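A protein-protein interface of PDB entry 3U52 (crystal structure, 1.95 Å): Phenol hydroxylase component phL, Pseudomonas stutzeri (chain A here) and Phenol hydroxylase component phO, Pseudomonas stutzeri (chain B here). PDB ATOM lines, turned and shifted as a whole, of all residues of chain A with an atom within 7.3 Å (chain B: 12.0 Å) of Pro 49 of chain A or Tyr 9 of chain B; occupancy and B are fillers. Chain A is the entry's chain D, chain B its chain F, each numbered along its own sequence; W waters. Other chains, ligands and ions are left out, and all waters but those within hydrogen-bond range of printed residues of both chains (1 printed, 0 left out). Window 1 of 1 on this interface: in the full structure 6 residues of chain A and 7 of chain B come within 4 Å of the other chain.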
ATOM      1  N   HIS A  46     -17.109  15.643 -10.414  1.00  0.00           N
ATOM      2  CA  HIS A  46     -16.080  14.615 -10.439  1.00  0.00           C
ATOM      3  C   HIS A  46     -16.171  13.627 -11.575  1.00  0.00           C
ATOM      4  O   HIS A  46     -15.161  12.998 -11.886  1.00  0.00           O
ATOM      5  CB  HIS A  46     -16.116  13.865  -9.111  1.00  0.00           C
ATOM      6  CG  HIS A  46     -15.537  14.676  -8.011  1.00  0.00           C
ATOM      7  ND1 HIS A  46     -16.259  15.653  -7.350  1.00  0.00           N
ATOM      8  CD2 HIS A  46     -14.278  14.743  -7.527  1.00  0.00           C
ATOM      9  CE1 HIS A  46     -15.484  16.242  -6.453  1.00  0.00           C
ATOM     10  NE2 HIS A  46     -14.275  15.719  -6.549  1.00  0.00           N
ATOM     11  N   TYR A  47     -17.371  13.433 -12.101  1.00  0.00           N
ATOM     12  CA  TYR A  47     -17.664  12.426 -13.123  1.00  0.00           C
ATOM     13  C   TYR A  47     -18.725  12.893 -14.115  1.00  0.00           C
ATOM     14  O   TYR A  47     -19.752  13.499 -13.724  1.00  0.00           O
ATOM     15  CB  TYR A  47     -18.155  11.096 -12.550  1.00  0.00           C
ATOM     16  CG  TYR A  47     -17.567  10.707 -11.222  1.00  0.00           C
ATOM     17  CD1 TYR A  47     -18.269  10.956 -10.040  1.00  0.00           C
ATOM     18  CD2 TYR A  47     -16.286  10.137 -11.137  1.00  0.00           C
ATOM     19  CE1 TYR A  47     -17.754  10.629  -8.848  1.00  0.00           C
ATOM     20  CE2 TYR A  47     -15.743   9.845  -9.946  1.00  0.00           C
ATOM     21  CZ  TYR A  47     -16.503  10.083  -8.785  1.00  0.00           C
ATOM     22  OH  TYR A  47     -15.997   9.773  -7.556  1.00  0.00           O
ATOM     23  N   ARG A  48     -18.520  12.532 -15.390  1.00  0.00           N
ATOM     24  CA  ARG A  48     -19.494  12.860 -16.436  1.00  0.00           C
ATOM     25  C   ARG A  48     -20.699  11.950 -16.315  1.00  0.00           C
ATOM     26  O   ARG A  48     -20.559  10.794 -16.049  1.00  0.00           O
ATOM     27  CB  ARG A  48     -18.865  12.698 -17.826  1.00  0.00           C
ATOM     28  CG  ARG A  48     -17.796  13.755 -18.137  1.00  0.00           C
ATOM     29  CD  ARG A  48     -18.388  15.071 -18.574  1.00  0.00           C
ATOM     30  NE  ARG A  48     -18.949  14.952 -19.906  1.00  0.00           N
ATOM     31  CZ  ARG A  48     -18.302  15.307 -21.002  1.00  0.00           C
ATOM     32  NH1 ARG A  48     -18.871  15.151 -22.196  1.00  0.00           N
ATOM     33  NH2 ARG A  48     -17.076  15.809 -20.897  1.00  0.00           N
ATOM     34  N   PRO A  49     -21.891  12.464 -16.578  1.00  0.00           N
ATOM     35  CA  PRO A  49     -23.091  11.625 -16.490  1.00  0.00           C
ATOM     36  C   PRO A  49     -23.035  10.398 -17.420  1.00  0.00           C
ATOM     37  O   PRO A  49     -22.647  10.518 -18.559  1.00  0.00           O
ATOM     38  CB  PRO A  49     -24.250  12.550 -16.924  1.00  0.00           C
ATOM     39  CG  PRO A  49     -23.683  13.968 -16.993  1.00  0.00           C
ATOM     40  CD  PRO A  49     -22.150  13.844 -17.044  1.00  0.00           C
ATOM     41  N   GLN A  50     -23.443   9.228 -16.932  1.00  0.00           N
ATOM     42  CA  GLN A  50     -23.581   8.018 -17.796  1.00  0.00           C
ATOM     43  C   GLN A  50     -24.759   8.135 -18.765  1.00  0.00           C
ATOM     44  O   GLN A  50     -24.915   7.338 -19.700  1.00  0.00           O
ATOM     45  CB  GLN A  50     -23.684   6.764 -16.905  1.00  0.00           C
ATOM     46  CG  GLN A  50     -22.385   6.573 -16.115  1.00  0.00           C
ATOM     47  CD  GLN A  50     -22.464   5.635 -14.935  1.00  0.00           C
ATOM     48  OE1 GLN A  50     -22.893   4.479 -15.035  1.00  0.00           O
ATOM     49  NE2 GLN A  50     -22.009   6.120 -13.796  1.00  0.00           N
ATOM     50  N   TRP A  51     -25.606   9.137 -18.550  1.00  0.00           N
ATOM     51  CA  TRP A  51     -26.895   9.247 -19.259  1.00  0.00           C
ATOM     52  C   TRP A  51     -26.955  10.460 -20.220  1.00  0.00           C
ATOM     53  O   TRP A  51     -27.986  10.716 -20.809  1.00  0.00           O
ATOM     54  CB  TRP A  51     -28.095   9.240 -18.253  1.00  0.00           C
ATOM     55  CG  TRP A  51     -27.782  10.056 -16.990  1.00  0.00           C
ATOM     56  CD1 TRP A  51     -27.313   9.577 -15.818  1.00  0.00           C
ATOM     57  CD2 TRP A  51     -27.843  11.468 -16.853  1.00  0.00           C
ATOM     58  NE1 TRP A  51     -27.064  10.611 -14.949  1.00  0.00           N
ATOM     59  CE2 TRP A  51     -27.394  11.784 -15.554  1.00  0.00           C
ATOM     60  CE3 TRP A  51     -28.229  12.511 -17.706  1.00  0.00           C
ATOM     61  CZ2 TRP A  51     -27.325  13.108 -15.069  1.00  0.00           C
ATOM     62  CZ3 TRP A  51     -28.134  13.850 -17.229  1.00  0.00           C
ATOM     63  CH2 TRP A  51     -27.689  14.117 -15.927  1.00  0.00           C
ATOM     64  N   ASP A  52     -25.848  11.180 -20.404  1.00  0.00           N
ATOM     65  CA  ASP A  52     -25.778  12.361 -21.288  1.00  0.00           C
ATOM     66  C   ASP A  52     -24.363  12.501 -21.860  1.00  0.00           C
ATOM     67  O   ASP A  52     -23.426  12.668 -21.096  1.00  0.00           O
ATOM     68  CB  ASP A  52     -26.065  13.631 -20.466  1.00  0.00           C
ATOM     69  CG  ASP A  52     -26.310  14.869 -21.316  1.00  0.00           C
ATOM     70  OD1 ASP A  52     -25.880  14.950 -22.490  1.00  0.00           O
ATOM     71  OD2 ASP A  52     -26.952  15.798 -20.779  1.00  0.00           O
ATOM     72  N   SER A  53     -24.204  12.490 -23.188  1.00  0.00           N
ATOM     73  CA  SER A  53     -22.843  12.630 -23.788  1.00  0.00           C
ATOM     74  C   SER A  53     -22.262  14.058 -23.871  1.00  0.00           C
ATOM     75  O   SER A  53     -21.056  14.228 -24.067  1.00  0.00           O
ATOM     76  CB  SER A  53     -22.769  11.957 -25.176  1.00  0.00           C
ATOM     77  OG  SER A  53     -23.868  12.308 -25.982  1.00  0.00           O
ATOM     78  N   GLU A  54     -23.115  15.054 -23.659  1.00  0.00           N
ATOM     79  CA  GLU A  54     -22.897  16.412 -24.107  1.00  0.00           C
ATOM     80  C   GLU A  54     -22.735  17.406 -22.955  1.00  0.00           C
ATOM     81  O   GLU A  54     -22.153  18.459 -23.146  1.00  0.00           O
ATOM     82  CB  GLU A  54     -24.075  16.888 -24.958  1.00  0.00           C
ATOM     83  CG  GLU A  54     -24.418  16.018 -26.160  1.00  0.00           C
ATOM     84  CD  GLU A  54     -23.365  16.078 -27.264  1.00  0.00           C
ATOM     85  OE1 GLU A  54     -23.310  17.120 -27.979  1.00  0.00           O
ATOM     86  OE2 GLU A  54     -22.601  15.081 -27.435  1.00  0.00           O
ATOM     87  N   HIS A  55     -23.283  17.105 -21.780  1.00  0.00           N
ATOM     88  CA  HIS A  55     -23.271  18.106 -20.719  1.00  0.00           C
ATOM     89  C   HIS A  55     -22.791  17.495 -19.424  1.00  0.00           C
ATOM     90  O   HIS A  55     -22.891  16.265 -19.221  1.00  0.00           O
ATOM     91  CB  HIS A  55     -24.666  18.714 -20.492  1.00  0.00           C
ATOM     92  CG  HIS A  55     -25.411  19.079 -21.734  1.00  0.00           C
ATOM     93  ND1 HIS A  55     -25.319  20.319 -22.319  1.00  0.00           N
ATOM     94  CD2 HIS A  55     -26.329  18.396 -22.458  1.00  0.00           C
ATOM     95  CE1 HIS A  55     -26.114  20.369 -23.371  1.00  0.00           C
ATOM     96  NE2 HIS A  55     -26.727  19.212 -23.481  1.00  0.00           N
ATOM     97  N   THR A  56     -22.219  18.330 -18.563  1.00  0.00           N
ATOM     98  CA  THR A  56     -21.808  17.900 -17.241  1.00  0.00           C
ATOM     99  C   THR A  56     -23.054  17.837 -16.319  1.00  0.00           C
ATOM    100  O   THR A  56     -24.147  18.119 -16.730  1.00  0.00           O
ATOM    101  CB  THR A  56     -20.754  18.832 -16.607  1.00  0.00           C
ATOM    102  OG1 THR A  56     -21.338  20.134 -16.378  1.00  0.00           O
ATOM    103  CG2 THR A  56     -19.526  18.968 -17.530  1.00  0.00           C
ATOM    104  N   LEU A  57     -22.859  17.427 -15.077  1.00  0.00           N
ATOM    105  CA  LEU A  57     -23.882  17.593 -14.063  1.00  0.00           C
ATOM    106  C   LEU A  57     -24.030  19.129 -13.913  1.00  0.00           C
ATOM    107  O   LEU A  57     -23.065  19.864 -14.155  1.00  0.00           O
ATOM    108  CB  LEU A  57     -23.345  16.975 -12.778  1.00  0.00           C
ATOM    109  CG  LEU A  57     -23.739  15.605 -12.213  1.00  0.00           C
ATOM    110  CD1 LEU A  57     -24.525  14.674 -13.132  1.00  0.00           C
ATOM    111  CD2 LEU A  57     -22.573  14.948 -11.448  1.00  0.00           C
ATOM    112  N   ASN A  58     -25.215  19.632 -13.556  1.00  0.00           N
ATOM    113  CA  ASN A  58     -25.380  21.112 -13.310  1.00  0.00           C
ATOM    114  C   ASN A  58     -24.780  22.014 -14.433  1.00  0.00           C
ATOM    115  O   ASN A  58     -23.862  22.843 -14.196  1.00  0.00           O
ATOM    116  CB  ASN A  58     -24.813  21.522 -11.925  1.00  0.00           C
ATOM    117  CG  ASN A  58     -25.508  20.802 -10.709  1.00  0.00           C
ATOM    118  OD1 ASN A  58     -26.305  19.865 -10.881  1.00  0.00           O
ATOM    119  ND2 ASN A  58     -25.196  21.258  -9.473  1.00  0.00           N
ATOM    120  N   ARG A  62     -27.579  23.080 -21.011  1.00  0.00           N
ATOM    121  CA  ARG A  62     -28.757  22.208 -21.302  1.00  0.00           C
ATOM    122  C   ARG A  62     -29.858  22.978 -21.990  1.00  0.00           C
ATOM    123  O   ARG A  62     -30.765  22.378 -22.574  1.00  0.00           O
ATOM    124  CB  ARG A  62     -29.336  21.486 -20.071  1.00  0.00           C
ATOM    125  CG  ARG A  62     -28.483  20.340 -19.621  1.00  0.00           C
ATOM    126  CD  ARG A  62     -29.147  19.331 -18.611  1.00  0.00           C
ATOM    127  NE  ARG A  62     -28.286  18.163 -18.646  1.00  0.00           N
ATOM    128  CZ  ARG A  62     -27.230  17.994 -17.875  1.00  0.00           C
ATOM    129  NH1 ARG A  62     -26.499  16.895 -18.040  1.00  0.00           N
ATOM    130  NH2 ARG A  62     -26.938  18.885 -16.904  1.00  0.00           N
ATOM    131  N   SER B   2     -17.256  -3.039 -16.074  1.00  0.00           N
ATOM    132  CA  SER B   2     -17.046  -1.808 -16.893  1.00  0.00           C
ATOM    133  C   SER B   2     -18.274  -0.904 -16.741  1.00  0.00           C
ATOM    134  O   SER B   2     -19.302  -1.371 -16.247  1.00  0.00           O
ATOM    135  CB  SER B   2     -16.818  -2.179 -18.350  1.00  0.00           C
ATOM    136  OG  SER B   2     -17.987  -2.775 -18.891  1.00  0.00           O
ATOM    137  N   VAL B   3     -18.173   0.363 -17.141  1.00  0.00           N
ATOM    138  CA  VAL B   3     -19.255   1.346 -16.926  1.00  0.00           C
ATOM    139  C   VAL B   3     -20.381   1.109 -17.932  1.00  0.00           C
ATOM    140  O   VAL B   3     -20.101   0.959 -19.110  1.00  0.00           O
ATOM    141  CB  VAL B   3     -18.740   2.812 -17.074  1.00  0.00           C
ATOM    142  CG1 VAL B   3     -19.868   3.845 -16.897  1.00  0.00           C
ATOM    143  CG2 VAL B   3     -17.686   3.110 -16.048  1.00  0.00           C
ATOM    144  N   ASN B   4     -21.640   1.095 -17.472  1.00  0.00           N
ATOM    145  CA  ASN B   4     -22.780   1.168 -18.366  1.00  0.00           C
ATOM    146  C   ASN B   4     -23.167   2.604 -18.572  1.00  0.00           C
ATOM    147  O   ASN B   4     -23.169   3.398 -17.620  1.00  0.00           O
ATOM    148  CB  ASN B   4     -23.988   0.443 -17.809  1.00  0.00           C
ATOM    149  CG  ASN B   4     -23.776  -1.034 -17.720  1.00  0.00           C
ATOM    150  OD1 ASN B   4     -22.948  -1.608 -18.420  1.00  0.00           O
ATOM    151  ND2 ASN B   4     -24.502  -1.657 -16.823  1.00  0.00           N
ATOM    152  N   ALA B   5     -23.532   2.923 -19.807  1.00  0.00           N
ATOM    153  CA  ALA B   5     -23.863   4.273 -20.192  1.00  0.00           C
ATOM    154  C   ALA B   5     -24.708   4.286 -21.470  1.00  0.00           C
ATOM    155  O   ALA B   5     -24.789   3.290 -22.212  1.00  0.00           O
ATOM    156  CB  ALA B   5     -22.597   5.098 -20.378  1.00  0.00           C
ATOM    157  N   LEU B   6     -25.289   5.440 -21.740  1.00  0.00           N
ATOM    158  CA  LEU B   6     -26.112   5.590 -22.923  1.00  0.00           C
ATOM    159  C   LEU B   6     -25.241   5.800 -24.176  1.00  0.00           C
ATOM    160  O   LEU B   6     -25.768   5.781 -25.276  1.00  0.00           O
ATOM    161  CB  LEU B   6     -27.085   6.746 -22.687  1.00  0.00           C
ATOM    162  CG  LEU B   6     -28.604   6.601 -22.837  1.00  0.00           C
ATOM    163  CD1 LEU B   6     -29.193   5.217 -22.613  1.00  0.00           C
ATOM    164  CD2 LEU B   6     -29.314   7.665 -21.962  1.00  0.00           C
ATOM    165  N   TYR B   7     -23.926   5.978 -24.000  1.00  0.00           N
ATOM    166  CA  TYR B   7     -23.008   6.342 -25.061  1.00  0.00           C
ATOM    167  C   TYR B   7     -21.672   5.697 -24.798  1.00  0.00           C
ATOM    168  O   TYR B   7     -21.514   5.067 -23.781  1.00  0.00           O
ATOM    169  CB  TYR B   7     -22.848   7.864 -25.124  1.00  0.00           C
ATOM    170  CG  TYR B   7     -22.311   8.560 -23.843  1.00  0.00           C
ATOM    171  CD1 TYR B   7     -23.142   8.836 -22.766  1.00  0.00           C
ATOM    172  CD2 TYR B   7     -20.997   8.997 -23.790  1.00  0.00           C
ATOM    173  CE1 TYR B   7     -22.625   9.517 -21.615  1.00  0.00           C
ATOM    174  CE2 TYR B   7     -20.494   9.640 -22.705  1.00  0.00           C
ATOM    175  CZ  TYR B   7     -21.295   9.891 -21.613  1.00  0.00           C
ATOM    176  OH  TYR B   7     -20.747  10.597 -20.574  1.00  0.00           O
ATOM    177  N   ASP B   8     -20.711   5.881 -25.695  1.00  0.00           N
ATOM    178  CA  ASP B   8     -19.359   5.333 -25.552  1.00  0.00           C
ATOM    179  C   ASP B   8     -18.596   6.137 -24.485  1.00  0.00           C
ATOM    180  O   ASP B   8     -18.130   7.269 -24.730  1.00  0.00           O
ATOM    181  CB  ASP B   8     -18.609   5.315 -26.897  1.00  0.00           C
ATOM    182  CG  ASP B   8     -17.203   4.714 -26.791  1.00  0.00           C
ATOM    183  OD1 ASP B   8     -17.055   3.632 -26.183  1.00  0.00           O
ATOM    184  OD2 ASP B   8     -16.256   5.363 -27.310  1.00  0.00           O
ATOM    185  N   TYR B   9     -18.523   5.544 -23.292  1.00  0.00           N
ATOM    186  CA  TYR B   9     -18.108   6.256 -22.063  1.00  0.00           C
ATOM    187  C   TYR B   9     -16.587   6.097 -21.877  1.00  0.00           C
ATOM    188  O   TYR B   9     -16.136   5.157 -21.233  1.00  0.00           O
ATOM    189  CB  TYR B   9     -18.923   5.711 -20.865  1.00  0.00           C
ATOM    190  CG  TYR B   9     -18.867   6.575 -19.602  1.00  0.00           C
ATOM    191  CD1 TYR B   9     -19.772   7.623 -19.404  1.00  0.00           C
ATOM    192  CD2 TYR B   9     -17.923   6.329 -18.605  1.00  0.00           C
ATOM    193  CE1 TYR B   9     -19.727   8.419 -18.213  1.00  0.00           C
ATOM    194  CE2 TYR B   9     -17.885   7.108 -17.398  1.00  0.00           C
ATOM    195  CZ  TYR B   9     -18.798   8.171 -17.246  1.00  0.00           C
ATOM    196  OH  TYR B   9     -18.766   8.982 -16.105  1.00  0.00           O
ATOM    197  N   LYS B  10     -15.809   6.966 -22.520  1.00  0.00           N
ATOM    198  CA  LYS B  10     -14.336   6.872 -22.529  1.00  0.00           C
ATOM    199  C   LYS B  10     -13.843   8.287 -22.372  1.00  0.00           C
ATOM    200  O   LYS B  10     -14.252   9.160 -23.120  1.00  0.00           O
ATOM    201  CB  LYS B  10     -13.827   6.348 -23.881  1.00  0.00           C
ATOM    202  CG  LYS B  10     -14.264   4.915 -24.205  1.00  0.00           C
ATOM    203  CD  LYS B  10     -13.618   3.925 -23.218  1.00  0.00           C
ATOM    204  CE  LYS B  10     -14.138   2.486 -23.412  1.00  0.00           C
ATOM    205  NZ  LYS B  10     -15.497   2.248 -22.815  1.00  0.00           N
ATOM    206  N   PHE B  11     -12.976   8.511 -21.402  1.00  0.00           N
ATOM    207  CA  PHE B  11     -12.454   9.839 -21.101  1.00  0.00           C
ATOM    208  C   PHE B  11     -10.949   9.710 -20.816  1.00  0.00           C
ATOM    209  O   PHE B  11     -10.452   8.624 -20.506  1.00  0.00           O
ATOM    210  CB  PHE B  11     -13.216  10.450 -19.894  1.00  0.00           C
ATOM    211  CG  PHE B  11     -14.676  10.686 -20.173  1.00  0.00           C
ATOM    212  CD1 PHE B  11     -15.086  11.848 -20.804  1.00  0.00           C
ATOM    213  CD2 PHE B  11     -15.615   9.723 -19.874  1.00  0.00           C
ATOM    214  CE1 PHE B  11     -16.433  12.051 -21.118  1.00  0.00           C
ATOM    215  CE2 PHE B  11     -16.961   9.931 -20.152  1.00  0.00           C
ATOM    216  CZ  PHE B  11     -17.377  11.069 -20.766  1.00  0.00           C
ATOM    217  N   GLU B  12     -10.229  10.812 -20.971  1.00  0.00           N
ATOM    218  CA  GLU B  12      -8.830  10.900 -20.612  1.00  0.00           C
ATOM    219  C   GLU B  12      -8.701  10.976 -19.070  1.00  0.00           C
ATOM    220  O   GLU B  12      -9.577  11.553 -18.419  1.00  0.00           O
ATOM    221  CB  GLU B  12      -8.267  12.156 -21.272  1.00  0.00           C
ATOM    222  CG  GLU B  12      -7.811  11.946 -22.716  1.00  0.00           C
ATOM    223  CD  GLU B  12      -6.424  11.270 -22.779  1.00  0.00           C
ATOM    224  OE1 GLU B  12      -6.350  10.016 -22.834  1.00  0.00           O
ATOM    225  OE2 GLU B  12      -5.396  12.002 -22.726  1.00  0.00           O
ATOM    226  N   PRO B  13      -7.675  10.324 -18.476  1.00  0.00           N
ATOM    227  CA  PRO B  13      -7.470  10.464 -17.037  1.00  0.00           C
ATOM    228  C   PRO B  13      -7.190  11.898 -16.714  1.00  0.00           C
ATOM    229  O   PRO B  13      -6.433  12.561 -17.439  1.00  0.00           O
ATOM    230  CB  PRO B  13      -6.220   9.641 -16.765  1.00  0.00           C
ATOM    231  CG  PRO B  13      -6.055   8.746 -17.960  1.00  0.00           C
ATOM    232  CD  PRO B  13      -6.724   9.378 -19.099  1.00  0.00           C
ATOM    233  N   LYS B  14      -7.781  12.398 -15.641  1.00  0.00           N
ATOM    234  CA  LYS B  14      -7.488  13.780 -15.242  1.00  0.00           C
ATOM    235  C   LYS B  14      -6.038  13.991 -14.802  1.00  0.00           C
ATOM    236  O   LYS B  14      -5.510  15.095 -14.925  1.00  0.00           O
ATOM    237  CB  LYS B  14      -8.452  14.232 -14.132  1.00  0.00           C
ATOM    238  CG  LYS B  14      -9.692  14.909 -14.682  1.00  0.00           C
ATOM    239  CD  LYS B  14     -10.099  15.987 -13.741  1.00  0.00           C
ATOM    240  CE  LYS B  14     -11.502  16.463 -14.061  1.00  0.00           C
ATOM    241  NZ  LYS B  14     -11.509  17.422 -15.152  1.00  0.00           N
HETATM  242  O   HOH W   1     -21.804   1.378 -14.434  1.00  0.00           O
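Of the 14 printed residues of chain A, 6 touch a printed residue of chain B. Hydrophobic or aromatic side chains of chain B within 4 Å of the printed part of chain A: Val 3, Ala 5, Leu 6, Tyr 7, Tyr 9 and Phe 11. Among the printed residues, 14 pairs touch across the chains.
Tyr 7 of chain B touches Arg 48 of chain A. CB of Arg 48 of chain A touches CZ of Phe 11 of chain B, 3.7 Å away. O of Pro 49 of chain A touches CE1 of Tyr 9 of chain B, at 3.6 Å. Val 3 of chain B touches Gln 50 of chain A. Gln 50 of chain A touches Ala 5 of chain B (O to CA, 3.3 Å). O of Gln 50 of chain A touches CE1 of Tyr 7 of chain B, at 3.7 Å. Tyr 9 of chain B touches Gln 50 of chain A (CE1 to CG, 3.9 Å). Trp 51 of chain A touches Leu 6 of chain B. CB of Ser 53 of chain A touches CG of Tyr 7 of chain B, 3.7 Å away.
His 46 of chain A touches none of the printed residues of chain B. Arg 48 of chain A touches just these residues of chain B: Tyr 7, Tyr 9 and Phe 11. Pro 49 of chain A touches just these residues of chain B: Tyr 7 and Tyr 9. Of chain B, only Val 3, Asn 4, Ala 5, Leu 6, Tyr 7 and Tyr 9 come within 4 Å of Gln 50 of chain A. Asp 52 of chain A touches just one residue of chain B: Tyr 7. Ser 53 of chain A touches one residue of chain B. Leu 57 of chain A touches none of the printed residues of chain B. Printed residues of chain A within 4 Å of Ala 5 of chain B: Gln 50. Of the printed residues of chain A, Leu 6 of chain B touches Gln 50 (2.8 Å) and Trp 51 (3.5 Å). Of chain A, only Arg 48, Pro 49 and Gln 50 come within 4 Å of Tyr 9 of chain B. Pro 13 of chain B touches none of the printed residues of chain A. The nearest printed residue of chain A that does not touch Asn 4 of chain B is Trp 51 of chain A (6.3 Å).
The side-chain hydroxyl (OG) of Ser 53 of chain A lies within hydrogen-bond range of the side-chain carboxylate (OE2) of Glu 54 of chain A, at 3.4 Å. NH1 of Arg 48 of chain A sits at hydrogen-bond distance from O of Ser 53 of chain A (3.0 Å). The side-chain carboxylate (OD2) of Asp 52 of chain A is in salt-bridge range of the guanidinium group (NH1) of Arg 62 of chain A. N of Glu 54 of chain A sits at hydrogen-bond distance from OD1 of Asp 52 of chain A (3.0 Å). The backbone NH (N) of His 55 of chain A sits at hydrogen-bond distance from the side-chain carboxylate (OD1) of Asp 52 of chain A.
Water W1 bridges the backbone NH (N) of Asn 4 of chain B (3.1 Å) and the side-chain amide oxygen (OE1) of Gln 50 of chain A (3.3 Å).
OE1 of Gln 50 of chain A lies close to O of Asn 4 of chain B, at 2.8 Å. N of Leu 6 of chain B is in hydrogen-bond range of O of Gln 50 of chain A, at 2.8 Å. OH of Tyr 7 of chain B sits close to O of Asp 52 of chain A (3.4 Å). O of Pro 49 of chain A lies within hydrogen-bond range of OH of Tyr 7 of chain B, at 2.8 Å. The backbone carbonyl oxygen of Arg 48 of chain A sits at hydrogen-bond distance from the side-chain hydroxyl of Tyr 9 of chain B (2.5 Å).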
